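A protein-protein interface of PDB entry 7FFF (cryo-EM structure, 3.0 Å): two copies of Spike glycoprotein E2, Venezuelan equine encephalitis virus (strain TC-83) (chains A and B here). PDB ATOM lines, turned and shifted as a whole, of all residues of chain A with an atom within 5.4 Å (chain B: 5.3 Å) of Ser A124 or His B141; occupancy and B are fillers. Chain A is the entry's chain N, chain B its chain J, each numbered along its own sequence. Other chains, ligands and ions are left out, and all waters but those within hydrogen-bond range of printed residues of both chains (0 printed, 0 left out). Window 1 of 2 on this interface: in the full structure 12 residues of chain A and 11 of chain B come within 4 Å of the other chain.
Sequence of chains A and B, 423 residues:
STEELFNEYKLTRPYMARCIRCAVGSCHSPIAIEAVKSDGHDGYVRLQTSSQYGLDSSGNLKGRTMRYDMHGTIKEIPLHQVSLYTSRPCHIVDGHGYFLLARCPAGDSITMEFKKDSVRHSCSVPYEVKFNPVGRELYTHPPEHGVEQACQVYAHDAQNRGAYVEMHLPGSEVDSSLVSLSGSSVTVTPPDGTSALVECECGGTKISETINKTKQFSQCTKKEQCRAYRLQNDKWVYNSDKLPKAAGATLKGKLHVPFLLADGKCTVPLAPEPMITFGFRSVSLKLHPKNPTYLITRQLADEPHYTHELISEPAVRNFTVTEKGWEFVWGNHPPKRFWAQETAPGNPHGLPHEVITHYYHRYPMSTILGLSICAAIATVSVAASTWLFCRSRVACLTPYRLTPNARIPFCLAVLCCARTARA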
ATOM      1  N   CYS A  19      -7.679   1.307  -6.785  1.00  0.00           N
ATOM      2  CA  CYS A  19      -6.439   2.067  -6.754  1.00  0.00           C
ATOM      3  C   CYS A  19      -6.760   3.502  -7.123  1.00  0.00           C
ATOM      4  O   CYS A  19      -7.847   3.785  -7.631  1.00  0.00           O
ATOM      5  CB  CYS A  19      -5.403   1.489  -7.713  1.00  0.00           C
ATOM      6  SG  CYS A  19      -3.773   2.233  -7.562  1.00  0.00           S
ATOM      7  N   ILE A  20      -5.828   4.413  -6.868  1.00  0.00           N
ATOM      8  CA  ILE A  20      -6.079   5.818  -7.162  1.00  0.00           C
ATOM      9  C   ILE A  20      -5.549   6.188  -8.531  1.00  0.00           C
ATOM     10  O   ILE A  20      -6.273   6.735  -9.360  1.00  0.00           O
ATOM     11  CB  ILE A  20      -5.427   6.705  -6.101  1.00  0.00           C
ATOM     12  CG1 ILE A  20      -5.644   6.133  -4.729  1.00  0.00           C
ATOM     13  CG2 ILE A  20      -6.053   8.078  -6.138  1.00  0.00           C
ATOM     14  CD1 ILE A  20      -4.633   6.663  -3.817  1.00  0.00           C
ATOM     15  N   ARG A  21      -4.270   5.945  -8.752  1.00  0.00           N
ATOM     16  CA  ARG A  21      -3.607   6.233 -10.013  1.00  0.00           C
ATOM     17  C   ARG A  21      -3.348   4.880 -10.658  1.00  0.00           C
ATOM     18  O   ARG A  21      -2.471   4.138 -10.211  1.00  0.00           O
ATOM     19  CB  ARG A  21      -2.308   7.002  -9.780  1.00  0.00           C
ATOM     20  CG  ARG A  21      -2.423   8.384  -9.139  1.00  0.00           C
ATOM     21  CD  ARG A  21      -2.985   9.358 -10.137  1.00  0.00           C
ATOM     22  NE  ARG A  21      -2.929  10.765  -9.753  1.00  0.00           N
ATOM     23  CZ  ARG A  21      -1.879  11.550  -9.980  1.00  0.00           C
ATOM     24  NH1 ARG A  21      -1.916  12.825  -9.642  1.00  0.00           N
ATOM     25  NH2 ARG A  21      -0.783  11.058 -10.530  1.00  0.00           N
ATOM     26  N   CYS A  22      -4.116   4.532 -11.684  1.00  0.00           N
ATOM     27  CA  CYS A  22      -3.922   3.271 -12.392  1.00  0.00           C
ATOM     28  C   CYS A  22      -3.779   3.520 -13.890  1.00  0.00           C
ATOM     29  O   CYS A  22      -4.495   2.969 -14.726  1.00  0.00           O
ATOM     30  CB  CYS A  22      -5.028   2.278 -12.053  1.00  0.00           C
ATOM     31  SG  CYS A  22      -6.692   2.799 -12.411  1.00  0.00           S
ATOM     32  N   SER A 109       6.038   7.645  -3.056  1.00  0.00           N
ATOM     33  CA  SER A 109       5.011   6.712  -3.478  1.00  0.00           C
ATOM     34  C   SER A 109       5.665   5.424  -3.953  1.00  0.00           C
ATOM     35  O   SER A 109       6.885   5.279  -3.916  1.00  0.00           O
ATOM     36  CB  SER A 109       4.154   7.330  -4.580  1.00  0.00           C
ATOM     37  OG  SER A 109       4.925   7.552  -5.742  1.00  0.00           O
ATOM     38  N   ILE A 110       4.835   4.474  -4.380  1.00  0.00           N
ATOM     39  CA  ILE A 110       5.268   3.257  -5.057  1.00  0.00           C
ATOM     40  C   ILE A 110       4.331   3.003  -6.220  1.00  0.00           C
ATOM     41  O   ILE A 110       3.110   3.024  -6.045  1.00  0.00           O
ATOM     42  CB  ILE A 110       5.290   2.033  -4.116  1.00  0.00           C
ATOM     43  CG1 ILE A 110       6.493   2.060  -3.195  1.00  0.00           C
ATOM     44  CG2 ILE A 110       5.284   0.728  -4.876  1.00  0.00           C
ATOM     45  CD1 ILE A 110       6.582   0.849  -2.314  1.00  0.00           C
ATOM     46  N   THR A 111       4.890   2.756  -7.399  1.00  0.00           N
ATOM     47  CA  THR A 111       4.119   2.339  -8.558  1.00  0.00           C
ATOM     48  C   THR A 111       4.554   0.946  -8.977  1.00  0.00           C
ATOM     49  O   THR A 111       5.611   0.792  -9.587  1.00  0.00           O
ATOM     50  CB  THR A 111       4.315   3.312  -9.714  1.00  0.00           C
ATOM     51  OG1 THR A 111       3.938   4.629  -9.300  1.00  0.00           O
ATOM     52  CG2 THR A 111       3.458   2.904 -10.892  1.00  0.00           C
ATOM     53  N   SER A 122      -1.216  -0.606 -13.725  1.00  0.00           N
ATOM     54  CA  SER A 122      -0.423   0.096 -12.731  1.00  0.00           C
ATOM     55  C   SER A 122      -1.253   0.314 -11.480  1.00  0.00           C
ATOM     56  O   SER A 122      -2.473   0.157 -11.484  1.00  0.00           O
ATOM     57  CB  SER A 122       0.074   1.443 -13.249  1.00  0.00           C
ATOM     58  OG  SER A 122       0.914   1.267 -14.367  1.00  0.00           O
ATOM     59  N   CYS A 123      -0.567   0.688 -10.404  1.00  0.00           N
ATOM     60  CA  CYS A 123      -1.205   1.217  -9.211  1.00  0.00           C
ATOM     61  C   CYS A 123      -0.184   2.037  -8.450  1.00  0.00           C
ATOM     62  O   CYS A 123       0.872   1.517  -8.087  1.00  0.00           O
ATOM     63  CB  CYS A 123      -1.745   0.112  -8.306  1.00  0.00           C
ATOM     64  SG  CYS A 123      -2.602   0.736  -6.850  1.00  0.00           S
ATOM     65  N   SER A 124      -0.496   3.307  -8.209  1.00  0.00           N
ATOM     66  CA  SER A 124       0.332   4.174  -7.385  1.00  0.00           C
ATOM     67  C   SER A 124      -0.422   4.497  -6.109  1.00  0.00           C
ATOM     68  O   SER A 124      -1.591   4.885  -6.156  1.00  0.00           O
ATOM     69  CB  SER A 124       0.687   5.463  -8.112  1.00  0.00           C
ATOM     70  OG  SER A 124       1.413   5.195  -9.291  1.00  0.00           O
ATOM     71  N   VAL A 125       0.238   4.327  -4.975  1.00  0.00           N
ATOM     72  CA  VAL A 125      -0.341   4.715  -3.695  1.00  0.00           C
ATOM     73  C   VAL A 125       0.616   5.688  -3.017  1.00  0.00           C
ATOM     74  O   VAL A 125       1.835   5.534  -3.135  1.00  0.00           O
ATOM     75  CB  VAL A 125      -0.638   3.492  -2.819  1.00  0.00           C
ATOM     76  CG1 VAL A 125      -1.825   2.750  -3.358  1.00  0.00           C
ATOM     77  CG2 VAL A 125       0.546   2.576  -2.803  1.00  0.00           C
ATOM     78  N   PRO A 126       0.124   6.702  -2.331  1.00  0.00           N
ATOM     79  CA  PRO A 126       1.039   7.687  -1.724  1.00  0.00           C
ATOM     80  C   PRO A 126       1.525   7.256  -0.344  1.00  0.00           C
ATOM     81  O   PRO A 126       1.132   7.787   0.696  1.00  0.00           O
ATOM     82  CB  PRO A 126       0.175   8.943  -1.678  1.00  0.00           C
ATOM     83  CG  PRO A 126      -1.187   8.439  -1.529  1.00  0.00           C
ATOM     84  CD  PRO A 126      -1.272   7.152  -2.280  1.00  0.00           C
ATOM     85  N   HIS B  91       2.692   9.256 -17.406  1.00  0.00           N
ATOM     86  CA  HIS B  91       1.673   8.366 -17.956  1.00  0.00           C
ATOM     87  C   HIS B  91       0.838   9.150 -18.955  1.00  0.00           C
ATOM     88  O   HIS B  91       0.119  10.071 -18.568  1.00  0.00           O
ATOM     89  CB  HIS B  91       0.792   7.784 -16.854  1.00  0.00           C
ATOM     90  CG  HIS B  91       1.502   6.820 -15.960  1.00  0.00           C
ATOM     91  ND1 HIS B  91       2.084   7.194 -14.771  1.00  0.00           N
ATOM     92  CD2 HIS B  91       1.738   5.495 -16.092  1.00  0.00           C
ATOM     93  CE1 HIS B  91       2.641   6.141 -14.204  1.00  0.00           C
ATOM     94  NE2 HIS B  91       2.446   5.096 -14.987  1.00  0.00           N
ATOM     95  N   PHE B 131       4.356  20.830 -10.146  1.00  0.00           N
ATOM     96  CA  PHE B 131       3.233  20.113  -9.561  1.00  0.00           C
ATOM     97  C   PHE B 131       2.563  21.013  -8.531  1.00  0.00           C
ATOM     98  O   PHE B 131       3.229  21.500  -7.615  1.00  0.00           O
ATOM     99  CB  PHE B 131       3.707  18.827  -8.898  1.00  0.00           C
ATOM    100  CG  PHE B 131       2.608  17.978  -8.365  1.00  0.00           C
ATOM    101  CD1 PHE B 131       1.931  17.118  -9.196  1.00  0.00           C
ATOM    102  CD2 PHE B 131       2.235  18.051  -7.037  1.00  0.00           C
ATOM    103  CE1 PHE B 131       0.916  16.337  -8.712  1.00  0.00           C
ATOM    104  CE2 PHE B 131       1.209  17.284  -6.555  1.00  0.00           C
ATOM    105  CZ  PHE B 131       0.556  16.420  -7.393  1.00  0.00           C
ATOM    106  N   TYR B 139       0.737  18.206  -0.430  1.00  0.00           N
ATOM    107  CA  TYR B 139       1.103  16.846  -0.772  1.00  0.00           C
ATOM    108  C   TYR B 139       1.970  16.851  -2.026  1.00  0.00           C
ATOM    109  O   TYR B 139       2.310  17.898  -2.577  1.00  0.00           O
ATOM    110  CB  TYR B 139      -0.146  15.976  -0.942  1.00  0.00           C
ATOM    111  CG  TYR B 139      -1.193  16.551  -1.859  1.00  0.00           C
ATOM    112  CD1 TYR B 139      -2.223  17.311  -1.355  1.00  0.00           C
ATOM    113  CD2 TYR B 139      -1.153  16.336  -3.226  1.00  0.00           C
ATOM    114  CE1 TYR B 139      -3.170  17.850  -2.175  1.00  0.00           C
ATOM    115  CE2 TYR B 139      -2.101  16.867  -4.055  1.00  0.00           C
ATOM    116  CZ  TYR B 139      -3.109  17.618  -3.518  1.00  0.00           C
ATOM    117  OH  TYR B 139      -4.064  18.154  -4.342  1.00  0.00           O
ATOM    118  N   THR B 140       2.352  15.659  -2.466  1.00  0.00           N
ATOM    119  CA  THR B 140       3.072  15.477  -3.717  1.00  0.00           C
ATOM    120  C   THR B 140       2.456  14.384  -4.573  1.00  0.00           C
ATOM    121  O   THR B 140       2.540  14.451  -5.803  1.00  0.00           O
ATOM    122  CB  THR B 140       4.545  15.156  -3.429  1.00  0.00           C
ATOM    123  OG1 THR B 140       5.047  16.113  -2.494  1.00  0.00           O
ATOM    124  CG2 THR B 140       5.399  15.270  -4.668  1.00  0.00           C
ATOM    125  N   HIS B 141       1.796  13.412  -3.968  1.00  0.00           N
ATOM    126  CA  HIS B 141       0.917  12.499  -4.640  1.00  0.00           C
ATOM    127  C   HIS B 141      -0.463  12.693  -4.031  1.00  0.00           C
ATOM    128  O   HIS B 141      -0.574  12.766  -2.800  1.00  0.00           O
ATOM    129  CB  HIS B 141       1.399  11.060  -4.445  1.00  0.00           C
ATOM    130  CG  HIS B 141       0.735  10.060  -5.335  1.00  0.00           C
ATOM    131  ND1 HIS B 141      -0.478   9.484  -5.035  1.00  0.00           N
ATOM    132  CD2 HIS B 141       1.132   9.511  -6.506  1.00  0.00           C
ATOM    133  CE1 HIS B 141      -0.806   8.634  -5.989  1.00  0.00           C
ATOM    134  NE2 HIS B 141       0.156   8.628  -6.890  1.00  0.00           N
ATOM    135  N   PRO B 142      -1.522  12.806  -4.840  1.00  0.00           N
ATOM    136  CA  PRO B 142      -2.834  13.132  -4.285  1.00  0.00           C
ATOM    137  C   PRO B 142      -3.378  11.981  -3.467  1.00  0.00           C
ATOM    138  O   PRO B 142      -3.097  10.805  -3.756  1.00  0.00           O
ATOM    139  CB  PRO B 142      -3.688  13.381  -5.541  1.00  0.00           C
ATOM    140  CG  PRO B 142      -3.054  12.559  -6.557  1.00  0.00           C
ATOM    141  CD  PRO B 142      -1.586  12.599  -6.288  1.00  0.00           C
ATOM    142  N   PRO B 143      -4.153  12.257  -2.427  1.00  0.00           N
ATOM    143  CA  PRO B 143      -4.410  11.256  -1.398  1.00  0.00           C
ATOM    144  C   PRO B 143      -5.477  10.263  -1.834  1.00  0.00           C
ATOM    145  O   PRO B 143      -6.039  10.345  -2.920  1.00  0.00           O
ATOM    146  CB  PRO B 143      -4.889  12.095  -0.222  1.00  0.00           C
ATOM    147  CG  PRO B 143      -5.557  13.220  -0.862  1.00  0.00           C
ATOM    148  CD  PRO B 143      -4.821  13.531  -2.112  1.00  0.00           C
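No position is printed for both chains.
Among the printed residues, pairs that only touch across the chains: Ile A20 with Pro B143 (3.9 Å), Arg A21 with His B141 (3.4 Å), Arg A21 with Pro B142 (3.3 Å), Ser A124 with His B141 (3.4 Å), Pro A126 with His B141 (3.5 Å) and Pro A126 with Pro B142 (3.8 Å).
Printed residues of chain B within 4 Å of Ile A20: Pro B143.
Printed residues of chain B within 4 Å of Arg A21: His B141 (3.4 Å) and Pro B142 (3.3 Å).
Cys A22 touches none of the printed residues of chain B.
Ser A124 touches just one residue of chain B: His B141 (3.4 Å).
Of the printed residues of chain B, Pro A126 touches His B141 and Pro B142.
Of chain A, only Arg A21, Ser A124 and Pro A126 come within 4 Å of His B141.
Of the printed residues of chain A, Pro B142 touches Arg A21 and Pro A126.
Of the printed residues of chain A, Pro B143 touches Ile A20 (3.9 Å).
The nearest residue of chain B that does not touch Ser A124 is His B91 (5.2 Å).
The nearest printed residue of chain B that does not touch Ile A20 is Pro B142 (4.4 Å).
SG of Cys A19 sits at hydrogen-bond distance from N of Ser A124 (3.5 Å).
The backbone NH of Ser A124 lies within hydrogen-bond range of the backbone carbonyl oxygen of Arg A21, at 2.9 Å.
OG1 of Thr A111 lies within hydrogen-bond range of OG of Ser A124 (2.6 Å).
The side-chain sulfur of Cys A19 forms a disulfide with the side-chain sulfur of Cys A123 (2.0 Å).
Of the 12 printed residues of chain A, 4 touch a printed residue of chain B.
Among the printed residues, 6 pairs touch across the chains.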
